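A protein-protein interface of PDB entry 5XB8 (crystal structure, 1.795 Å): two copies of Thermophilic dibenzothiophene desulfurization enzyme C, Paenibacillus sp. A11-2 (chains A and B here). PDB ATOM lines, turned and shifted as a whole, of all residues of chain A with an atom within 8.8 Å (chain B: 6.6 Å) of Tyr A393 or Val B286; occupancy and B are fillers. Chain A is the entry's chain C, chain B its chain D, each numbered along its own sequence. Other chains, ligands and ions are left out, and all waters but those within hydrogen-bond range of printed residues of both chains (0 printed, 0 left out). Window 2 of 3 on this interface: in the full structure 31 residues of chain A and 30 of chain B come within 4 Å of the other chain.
The side-chain carboxylate (OD1) of Asp B292 lies within hydrogen-bond range of the side-chain hydroxyl (OH) of Tyr A393 (2.6 Å).
Of the 12 printed residues of chain B, 4 touch a printed residue of chain A.
Hydrophobic or aromatic side chains of chain B that line the printed part of chain A: Phe B281, Val B286 and Tyr B294.
Of the 21 printed residues of chain A, 4 touch a printed residue of chain B.
Among the printed residues, no Asp or Glu carboxylate lies within 4 Å of a Lys or Arg side-chain nitrogen of the other chain.
Of the printed residues of chain B, Tyr A393 touches Phe B281, Val B286, Asp B292 and Tyr B294.
Val B286 touches just one residue of chain A: Tyr A393.
Of the printed residues of chain B, Pro A390 touches Phe B281.
Of the printed residues of chain A, Phe B281 touches Pro A390 (3.4 Å) and Tyr A393 (3.7 Å).
Printed residues of chain A within 4 Å of Tyr B294: Ala A392 (3.7 Å), Tyr A393 (3.7 Å) and Arg A396 (3.6 Å).
Of the printed residues of chain B, Arg A396 touches Tyr B294 (3.6 Å).
Of the printed residues of chain A, Asp B292 touches Tyr A393 (2.6 Å).
Ala B289 touches none of the printed residues of chain A.
Among the printed residues, pairs that only touch across the chains: Pro A390 with Phe B281 (3.4 Å), Ala A392 with Tyr B294 (3.7 Å), Tyr A393 with Phe B281 (3.7 Å), Tyr A393 with Val B286 (3.5 Å), Tyr A393 with Tyr B294 (3.7 Å) and Arg A396 with Tyr B294 (3.6 Å).
No position is printed for both chains.
N of Tyr B294 lies within hydrogen-bond range of OD2 of Asp B292 (2.8 Å).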
ATOM      1  N   GLN A 252     -26.264  22.738 -17.752  1.00  0.00           N
ATOM      2  CA  GLN A 252     -25.112  21.865 -17.550  1.00  0.00           C
ATOM      3  C   GLN A 252     -24.817  21.040 -18.790  1.00  0.00           C
ATOM      4  O   GLN A 252     -23.650  20.726 -19.056  1.00  0.00           O
ATOM      5  CB  GLN A 252     -25.355  20.989 -16.327  1.00  0.00           C
ATOM      6  CG  GLN A 252     -25.331  21.789 -15.012  1.00  0.00           C
ATOM      7  CD  GLN A 252     -23.913  22.100 -14.526  1.00  0.00           C
ATOM      8  OE1 GLN A 252     -23.026  21.273 -14.659  1.00  0.00           O
ATOM      9  NE2 GLN A 252     -23.699  23.296 -13.956  1.00  0.00           N
ATOM     10  N   MET A 338     -30.968  14.933 -14.879  1.00  0.00           N
ATOM     11  CA  MET A 338     -29.829  15.630 -14.295  1.00  0.00           C
ATOM     12  C   MET A 338     -28.665  14.672 -14.064  1.00  0.00           C
ATOM     13  O   MET A 338     -27.501  15.034 -14.274  1.00  0.00           O
ATOM     14  CB  MET A 338     -30.247  16.303 -12.993  1.00  0.00           C
ATOM     15  CG  MET A 338     -29.189  17.161 -12.342  1.00  0.00           C
ATOM     16  SD  MET A 338     -28.739  18.654 -13.283  1.00  0.00           S
ATOM     17  CE  MET A 338     -27.049  18.287 -13.736  1.00  0.00           C
ATOM     18  N   ALA A 342     -25.146  15.211 -15.680  1.00  0.00           N
ATOM     19  CA  ALA A 342     -23.946  15.233 -14.847  1.00  0.00           C
ATOM     20  C   ALA A 342     -22.957  14.169 -15.288  1.00  0.00           C
ATOM     21  O   ALA A 342     -21.749  14.429 -15.361  1.00  0.00           O
ATOM     22  CB  ALA A 342     -24.307  15.035 -13.379  1.00  0.00           C
ATOM     23  N   LYS A 345     -21.278  15.341 -18.393  1.00  0.00           N
ATOM     24  CA  LYS A 345     -20.343  16.423 -18.094  1.00  0.00           C
ATOM     25  C   LYS A 345     -19.058  15.896 -17.457  1.00  0.00           C
ATOM     26  O   LYS A 345     -17.965  16.400 -17.752  1.00  0.00           O
ATOM     27  CB  LYS A 345     -20.998  17.436 -17.176  1.00  0.00           C
ATOM     28  CG  LYS A 345     -20.219  18.730 -17.078  1.00  0.00           C
ATOM     29  CD  LYS A 345     -20.688  19.535 -15.896  1.00  0.00           C
ATOM     30  CE  LYS A 345     -20.020  20.872 -15.839  1.00  0.00           C
ATOM     31  NZ  LYS A 345     -20.319  21.501 -14.528  1.00  0.00           N
ATOM     32  N   ILE A 346     -19.184  14.933 -16.547  1.00  0.00           N
ATOM     33  CA  ILE A 346     -18.024  14.319 -15.894  1.00  0.00           C
ATOM     34  C   ILE A 346     -17.107  13.705 -16.941  1.00  0.00           C
ATOM     35  O   ILE A 346     -15.895  13.954 -16.963  1.00  0.00           O
ATOM     36  CB  ILE A 346     -18.479  13.261 -14.867  1.00  0.00           C
ATOM     37  CG1 ILE A 346     -19.213  13.899 -13.675  1.00  0.00           C
ATOM     38  CG2 ILE A 346     -17.285  12.435 -14.362  1.00  0.00           C
ATOM     39  CD1 ILE A 346     -20.108  12.944 -12.923  1.00  0.00           C
ATOM     40  N   ARG A 350     -13.257  15.115 -17.936  1.00  0.00           N
ATOM     41  CA  ARG A 350     -12.026  14.335 -17.859  1.00  0.00           C
ATOM     42  C   ARG A 350     -11.386  14.206 -19.222  1.00  0.00           C
ATOM     43  O   ARG A 350     -10.159  14.337 -19.367  1.00  0.00           O
ATOM     44  CB  ARG A 350     -12.313  12.955 -17.285  1.00  0.00           C
ATOM     45  CG  ARG A 350     -12.921  12.987 -15.897  1.00  0.00           C
ATOM     46  CD  ARG A 350     -12.074  13.788 -14.942  1.00  0.00           C
ATOM     47  NE  ARG A 350     -12.376  13.490 -13.540  1.00  0.00           N
ATOM     48  CZ  ARG A 350     -11.991  14.258 -12.526  1.00  0.00           C
ATOM     49  NH1 ARG A 350     -11.299  15.369 -12.765  1.00  0.00           N
ATOM     50  NH2 ARG A 350     -12.296  13.923 -11.278  1.00  0.00           N
ATOM     51  N   ASP A 389     -18.206  24.897 -11.984  1.00  0.00           N
ATOM     52  CA  ASP A 389     -18.598  24.263 -10.742  1.00  0.00           C
ATOM     53  C   ASP A 389     -17.814  22.962 -10.641  1.00  0.00           C
ATOM     54  O   ASP A 389     -17.385  22.410 -11.664  1.00  0.00           O
ATOM     55  CB  ASP A 389     -20.114  24.027 -10.659  1.00  0.00           C
ATOM     56  CG  ASP A 389     -20.659  23.241 -11.822  1.00  0.00           C
ATOM     57  OD1 ASP A 389     -20.985  23.853 -12.865  1.00  0.00           O
ATOM     58  OD2 ASP A 389     -20.769  22.010 -11.680  1.00  0.00           O
ATOM     59  N   PRO A 390     -17.531  22.506  -9.429  1.00  0.00           N
ATOM     60  CA  PRO A 390     -16.520  21.453  -9.266  1.00  0.00           C
ATOM     61  C   PRO A 390     -17.027  20.090  -9.712  1.00  0.00           C
ATOM     62  O   PRO A 390     -18.078  19.611  -9.274  1.00  0.00           O
ATOM     63  CB  PRO A 390     -16.208  21.487  -7.763  1.00  0.00           C
ATOM     64  CG  PRO A 390     -17.409  22.111  -7.137  1.00  0.00           C
ATOM     65  CD  PRO A 390     -17.947  23.080  -8.141  1.00  0.00           C
ATOM     66  N   VAL A 391     -16.240  19.449 -10.575  1.00  0.00           N
ATOM     67  CA  VAL A 391     -16.619  18.148 -11.099  1.00  0.00           C
ATOM     68  C   VAL A 391     -16.673  17.127  -9.984  1.00  0.00           C
ATOM     69  O   VAL A 391     -17.394  16.136 -10.090  1.00  0.00           O
ATOM     70  CB  VAL A 391     -15.656  17.718 -12.224  1.00  0.00           C
ATOM     71  CG1 VAL A 391     -14.258  17.328 -11.673  1.00  0.00           C
ATOM     72  CG2 VAL A 391     -16.262  16.594 -13.029  1.00  0.00           C
ATOM     73  N   ALA A 392     -15.925  17.346  -8.891  1.00  0.00           N
ATOM     74  CA  ALA A 392     -15.953  16.381  -7.796  1.00  0.00           C
ATOM     75  C   ALA A 392     -17.346  16.259  -7.211  1.00  0.00           C
ATOM     76  O   ALA A 392     -17.748  15.178  -6.766  1.00  0.00           O
ATOM     77  CB  ALA A 392     -14.970  16.781  -6.691  1.00  0.00           C
ATOM     78  N   TYR A 393     -18.098  17.353  -7.192  1.00  0.00           N
ATOM     79  CA  TYR A 393     -19.441  17.302  -6.638  1.00  0.00           C
ATOM     80  C   TYR A 393     -20.477  16.832  -7.650  1.00  0.00           C
ATOM     81  O   TYR A 393     -21.494  16.260  -7.251  1.00  0.00           O
ATOM     82  CB  TYR A 393     -19.799  18.657  -6.028  1.00  0.00           C
ATOM     83  CG  TYR A 393     -19.082  18.761  -4.716  1.00  0.00           C
ATOM     84  CD1 TYR A 393     -19.592  18.135  -3.585  1.00  0.00           C
ATOM     85  CD2 TYR A 393     -17.842  19.382  -4.623  1.00  0.00           C
ATOM     86  CE1 TYR A 393     -18.907  18.159  -2.389  1.00  0.00           C
ATOM     87  CE2 TYR A 393     -17.148  19.414  -3.437  1.00  0.00           C
ATOM     88  CZ  TYR A 393     -17.686  18.802  -2.318  1.00  0.00           C
ATOM     89  OH  TYR A 393     -17.012  18.807  -1.128  1.00  0.00           O
ATOM     90  N   LYS A 394     -20.227  17.003  -8.944  1.00  0.00           N
ATOM     91  CA  LYS A 394     -21.005  16.269  -9.940  1.00  0.00           C
ATOM     92  C   LYS A 394     -20.837  14.763  -9.762  1.00  0.00           C
ATOM     93  O   LYS A 394     -21.815  14.004  -9.806  1.00  0.00           O
ATOM     94  CB  LYS A 394     -20.598  16.693 -11.344  1.00  0.00           C
ATOM     95  CG  LYS A 394     -21.089  18.096 -11.715  1.00  0.00           C
ATOM     96  CD  LYS A 394     -22.582  18.092 -12.016  1.00  0.00           C
ATOM     97  CE  LYS A 394     -23.210  19.468 -11.785  1.00  0.00           C
ATOM     98  NZ  LYS A 394     -23.299  19.824 -10.344  1.00  0.00           N
ATOM     99  N   ILE A 395     -19.593  14.314  -9.595  1.00  0.00           N
ATOM    100  CA  ILE A 395     -19.312  12.907  -9.306  1.00  0.00           C
ATOM    101  C   ILE A 395     -20.056  12.456  -8.053  1.00  0.00           C
ATOM    102  O   ILE A 395     -20.704  11.402  -8.034  1.00  0.00           O
ATOM    103  CB  ILE A 395     -17.784  12.704  -9.186  1.00  0.00           C
ATOM    104  CG1 ILE A 395     -17.129  12.873 -10.561  1.00  0.00           C
ATOM    105  CG2 ILE A 395     -17.450  11.345  -8.611  1.00  0.00           C
ATOM    106  CD1 ILE A 395     -15.606  13.010 -10.524  1.00  0.00           C
ATOM    107  N   ARG A 396     -19.984  13.253  -6.987  1.00  0.00           N
ATOM    108  CA  ARG A 396     -20.672  12.882  -5.752  1.00  0.00           C
ATOM    109  C   ARG A 396     -22.175  12.779  -5.976  1.00  0.00           C
ATOM    110  O   ARG A 396     -22.823  11.857  -5.466  1.00  0.00           O
ATOM    111  CB  ARG A 396     -20.367  13.891  -4.641  1.00  0.00           C
ATOM    112  CG  ARG A 396     -20.841  13.430  -3.256  1.00  0.00           C
ATOM    113  CD  ARG A 396     -20.844  14.555  -2.237  1.00  0.00           C
ATOM    114  NE  ARG A 396     -21.134  14.073  -0.887  1.00  0.00           N
ATOM    115  CZ  ARG A 396     -22.352  13.816  -0.417  1.00  0.00           C
ATOM    116  NH1 ARG A 396     -22.511  13.388   0.835  1.00  0.00           N
ATOM    117  NH2 ARG A 396     -23.414  13.984  -1.189  1.00  0.00           N
ATOM    118  N   GLU A 397     -22.749  13.711  -6.750  1.00  0.00           N
ATOM    119  CA  GLU A 397     -24.176  13.658  -7.048  1.00  0.00           C
ATOM    120  C   GLU A 397     -24.548  12.389  -7.809  1.00  0.00           C
ATOM    121  O   GLU A 397     -25.574  11.760  -7.519  1.00  0.00           O
ATOM    122  CB  GLU A 397     -24.592  14.916  -7.818  1.00  0.00           C
ATOM    123  CG  GLU A 397     -24.521  16.139  -6.947  1.00  0.00           C
ATOM    124  CD  GLU A 397     -24.307  17.444  -7.707  1.00  0.00           C
ATOM    125  OE1 GLU A 397     -24.281  17.454  -8.956  1.00  0.00           O
ATOM    126  OE2 GLU A 397     -24.146  18.472  -7.022  1.00  0.00           O
ATOM    127  N   VAL A 398     -23.738  11.988  -8.788  1.00  0.00           N
ATOM    128  CA  VAL A 398     -24.041  10.743  -9.488  1.00  0.00           C
ATOM    129  C   VAL A 398     -23.889   9.556  -8.541  1.00  0.00           C
ATOM    130  O   VAL A 398     -24.677   8.602  -8.584  1.00  0.00           O
ATOM    131  CB  VAL A 398     -23.166  10.591 -10.745  1.00  0.00           C
ATOM    132  CG1 VAL A 398     -23.377   9.215 -11.386  1.00  0.00           C
ATOM    133  CG2 VAL A 398     -23.518  11.684 -11.754  1.00  0.00           C
ATOM    134  N   GLY A 399     -22.886   9.593  -7.665  1.00  0.00           N
ATOM    135  CA  GLY A 399     -22.683   8.472  -6.754  1.00  0.00           C
ATOM    136  C   GLY A 399     -23.784   8.372  -5.722  1.00  0.00           C
ATOM    137  O   GLY A 399     -24.224   7.277  -5.371  1.00  0.00           O
ATOM    138  N   ASN A 400     -24.248   9.516  -5.233  1.00  0.00           N
ATOM    139  CA  ASN A 400     -25.341   9.542  -4.271  1.00  0.00           C
ATOM    140  C   ASN A 400     -26.618   8.997  -4.901  1.00  0.00           C
ATOM    141  O   ASN A 400     -27.401   8.295  -4.245  1.00  0.00           O
ATOM    142  CB  ASN A 400     -25.525  10.978  -3.779  1.00  0.00           C
ATOM    143  CG  ASN A 400     -26.183  11.071  -2.416  1.00  0.00           C
ATOM    144  OD1 ASN A 400     -26.225  10.105  -1.644  1.00  0.00           O
ATOM    145  ND2 ASN A 400     -26.664  12.258  -2.098  1.00  0.00           N
ATOM    146  N   PRO A 408     -30.185  14.514  -7.242  1.00  0.00           N
ATOM    147  CA  PRO A 408     -29.571  15.746  -6.763  1.00  0.00           C
ATOM    148  C   PRO A 408     -30.635  16.757  -6.382  1.00  0.00           C
ATOM    149  O   PRO A 408     -31.704  16.831  -6.992  1.00  0.00           O
ATOM    150  CB  PRO A 408     -28.727  16.225  -7.949  1.00  0.00           C
ATOM    151  CG  PRO A 408     -29.172  15.484  -9.085  1.00  0.00           C
ATOM    152  CD  PRO A 408     -29.793  14.210  -8.624  1.00  0.00           C
ATOM    153  N   TYR A 413     -26.772  24.806  -9.703  1.00  0.00           N
ATOM    154  CA  TYR A 413     -25.667  23.968 -10.147  1.00  0.00           C
ATOM    155  C   TYR A 413     -26.004  22.487 -10.225  1.00  0.00           C
ATOM    156  O   TYR A 413     -25.200  21.723 -10.773  1.00  0.00           O
ATOM    157  CB  TYR A 413     -24.462  24.142  -9.206  1.00  0.00           C
ATOM    158  CG  TYR A 413     -23.923  25.549  -9.174  1.00  0.00           C
ATOM    159  CD1 TYR A 413     -24.308  26.443  -8.174  1.00  0.00           C
ATOM    160  CD2 TYR A 413     -23.043  26.000 -10.149  1.00  0.00           C
ATOM    161  CE1 TYR A 413     -23.819  27.731  -8.139  1.00  0.00           C
ATOM    162  CE2 TYR A 413     -22.544  27.289 -10.118  1.00  0.00           C
ATOM    163  CZ  TYR A 413     -22.935  28.149  -9.113  1.00  0.00           C
ATOM    164  OH  TYR A 413     -22.446  29.432  -9.085  1.00  0.00           O
ATOM    165  N   SER A 414     -27.146  22.055  -9.700  1.00  0.00           N
ATOM    166  CA  SER A 414     -27.530  20.649  -9.724  1.00  0.00           C
ATOM    167  C   SER A 414     -29.041  20.493  -9.803  1.00  0.00           C
ATOM    168  O   SER A 414     -29.787  21.470 -10.010  1.00  0.00           O
ATOM    169  CB  SER A 414     -26.993  19.939  -8.478  1.00  0.00           C
ATOM    170  OG  SER A 414     -27.524  20.532  -7.307  1.00  0.00           O
ATOM    171  OXT SER A 414     -29.523  19.362  -9.681  1.00  0.00           O
ATOM    172  N   PRO B 280     -14.825  27.672   0.012  1.00  0.00           N
ATOM    173  CA  PRO B 280     -15.462  26.364   0.181  1.00  0.00           C
ATOM    174  C   PRO B 280     -16.678  26.243  -0.714  1.00  0.00           C
ATOM    175  O   PRO B 280     -17.301  27.239  -1.089  1.00  0.00           O
ATOM    176  CB  PRO B 280     -15.853  26.347   1.661  1.00  0.00           C
ATOM    177  CG  PRO B 280     -16.042  27.801   2.002  1.00  0.00           C
ATOM    178  CD  PRO B 280     -15.039  28.552   1.173  1.00  0.00           C
ATOM    179  N   PHE B 281     -17.010  25.007  -1.069  1.00  0.00           N
ATOM    180  CA  PHE B 281     -18.182  24.753  -1.895  1.00  0.00           C
ATOM    181  C   PHE B 281     -19.315  24.219  -1.024  1.00  0.00           C
ATOM    182  O   PHE B 281     -19.809  24.927  -0.151  1.00  0.00           O
ATOM    183  CB  PHE B 281     -17.840  23.774  -3.019  1.00  0.00           C
ATOM    184  CG  PHE B 281     -18.957  23.561  -4.004  1.00  0.00           C
ATOM    185  CD1 PHE B 281     -19.192  24.476  -5.019  1.00  0.00           C
ATOM    186  CD2 PHE B 281     -19.761  22.439  -3.918  1.00  0.00           C
ATOM    187  CE1 PHE B 281     -20.213  24.279  -5.928  1.00  0.00           C
ATOM    188  CE2 PHE B 281     -20.778  22.235  -4.819  1.00  0.00           C
ATOM    189  CZ  PHE B 281     -21.009  23.157  -5.829  1.00  0.00           C
ATOM    190  N   GLY B 285     -21.686  21.498   1.848  1.00  0.00           N
ATOM    191  CA  GLY B 285     -21.660  21.785   3.272  1.00  0.00           C
ATOM    192  C   GLY B 285     -20.255  21.830   3.837  1.00  0.00           C
ATOM    193  O   GLY B 285     -20.002  21.352   4.941  1.00  0.00           O
ATOM    194  N   VAL B 286     -19.348  22.414   3.061  1.00  0.00           N
ATOM    195  CA  VAL B 286     -17.954  22.583   3.448  1.00  0.00           C
ATOM    196  C   VAL B 286     -17.781  23.964   4.067  1.00  0.00           C
ATOM    197  O   VAL B 286     -18.263  24.962   3.518  1.00  0.00           O
ATOM    198  CB  VAL B 286     -17.028  22.417   2.229  1.00  0.00           C
ATOM    199  CG1 VAL B 286     -15.569  22.479   2.658  1.00  0.00           C
ATOM    200  CG2 VAL B 286     -17.327  21.116   1.493  1.00  0.00           C
ATOM    201  N   GLU B 287     -17.070  24.031   5.191  1.00  0.00           N
ATOM    202  CA  GLU B 287     -16.799  25.308   5.848  1.00  0.00           C
ATOM    203  C   GLU B 287     -15.483  25.934   5.402  1.00  0.00           C
ATOM    204  O   GLU B 287     -15.392  27.165   5.301  1.00  0.00           O
ATOM    205  CB  GLU B 287     -16.792  25.123   7.370  1.00  0.00           C
ATOM    206  N   LYS B 288     -14.469  25.122   5.099  1.00  0.00           N
ATOM    207  CA  LYS B 288     -13.175  25.623   4.654  1.00  0.00           C
ATOM    208  C   LYS B 288     -12.689  24.757   3.503  1.00  0.00           C
ATOM    209  O   LYS B 288     -12.811  23.532   3.555  1.00  0.00           O
ATOM    210  CB  LYS B 288     -12.146  25.607   5.801  1.00  0.00           C
ATOM    211  N   ALA B 289     -12.135  25.394   2.467  1.00  0.00           N
ATOM    212  CA  ALA B 289     -11.673  24.637   1.310  1.00  0.00           C
ATOM    213  C   ALA B 289     -10.549  23.685   1.686  1.00  0.00           C
ATOM    214  O   ALA B 289     -10.409  22.616   1.085  1.00  0.00           O
ATOM    215  CB  ALA B 289     -11.209  25.590   0.211  1.00  0.00           C
ATOM    216  N   THR B 290      -9.738  24.060   2.675  1.00  0.00           N
ATOM    217  CA  THR B 290      -8.633  23.217   3.116  1.00  0.00           C
ATOM    218  C   THR B 290      -9.101  21.985   3.884  1.00  0.00           C
ATOM    219  O   THR B 290      -8.268  21.133   4.205  1.00  0.00           O
ATOM    220  CB  THR B 290      -7.662  24.030   3.982  1.00  0.00           C
ATOM    221  OG1 THR B 290      -8.378  24.626   5.066  1.00  0.00           O
ATOM    222  CG2 THR B 290      -6.985  25.121   3.172  1.00  0.00           C
ATOM    223  N   GLU B 291     -10.393  21.882   4.202  1.00  0.00           N
ATOM    224  CA  GLU B 291     -10.970  20.678   4.783  1.00  0.00           C
ATOM    225  C   GLU B 291     -11.847  19.920   3.795  1.00  0.00           C
ATOM    226  O   GLU B 291     -12.459  18.923   4.172  1.00  0.00           O
ATOM    227  CB  GLU B 291     -11.806  21.024   6.028  1.00  0.00           C
ATOM    228  CG  GLU B 291     -10.998  21.614   7.195  1.00  0.00           C
ATOM    229  CD  GLU B 291      -9.969  20.641   7.756  1.00  0.00           C
ATOM    230  OE1 GLU B 291      -8.840  21.092   8.063  1.00  0.00           O
ATOM    231  OE2 GLU B 291     -10.285  19.430   7.888  1.00  0.00           O
ATOM    232  N   ASP B 292     -11.931  20.366   2.552  1.00  0.00           N
ATOM    233  CA  ASP B 292     -12.759  19.676   1.578  1.00  0.00           C
ATOM    234  C   ASP B 292     -12.150  18.305   1.285  1.00  0.00           C
ATOM    235  O   ASP B 292     -10.948  18.212   1.018  1.00  0.00           O
ATOM    236  CB  ASP B 292     -12.872  20.512   0.306  1.00  0.00           C
ATOM    237  CG  ASP B 292     -13.748  19.859  -0.750  1.00  0.00           C
ATOM    238  OD1 ASP B 292     -14.910  20.285  -0.918  1.00  0.00           O
ATOM    239  OD2 ASP B 292     -13.277  18.910  -1.412  1.00  0.00           O
ATOM    240  N   PRO B 293     -12.928  17.219   1.350  1.00  0.00           N
ATOM    241  CA  PRO B 293     -12.319  15.893   1.177  1.00  0.00           C
ATOM    242  C   PRO B 293     -11.717  15.694  -0.198  1.00  0.00           C
ATOM    243  O   PRO B 293     -10.722  14.972  -0.336  1.00  0.00           O
ATOM    244  CB  PRO B 293     -13.490  14.932   1.441  1.00  0.00           C
ATOM    245  CG  PRO B 293     -14.714  15.731   1.061  1.00  0.00           C
ATOM    246  CD  PRO B 293     -14.392  17.141   1.507  1.00  0.00           C
ATOM    247  N   TYR B 294     -12.272  16.328  -1.227  1.00  0.00           N
ATOM    248  CA  TYR B 294     -11.743  16.111  -2.574  1.00  0.00           C
ATOM    249  C   TYR B 294     -10.532  16.986  -2.858  1.00  0.00           C
ATOM    250  O   TYR B 294      -9.631  16.575  -3.609  1.00  0.00           O
ATOM    251  CB  TYR B 294     -12.856  16.343  -3.601  1.00  0.00           C
ATOM    252  CG  TYR B 294     -14.060  15.485  -3.290  1.00  0.00           C
ATOM    253  CD1 TYR B 294     -13.936  14.109  -3.214  1.00  0.00           C
ATOM    254  CD2 TYR B 294     -15.299  16.044  -3.032  1.00  0.00           C
ATOM    255  CE1 TYR B 294     -15.031  13.297  -2.918  1.00  0.00           C
ATOM    256  CE2 TYR B 294     -16.408  15.229  -2.731  1.00  0.00           C
ATOM    257  CZ  TYR B 294     -16.255  13.864  -2.677  1.00  0.00           C
ATOM    258  OH  TYR B 294     -17.330  13.045  -2.378  1.00  0.00           O
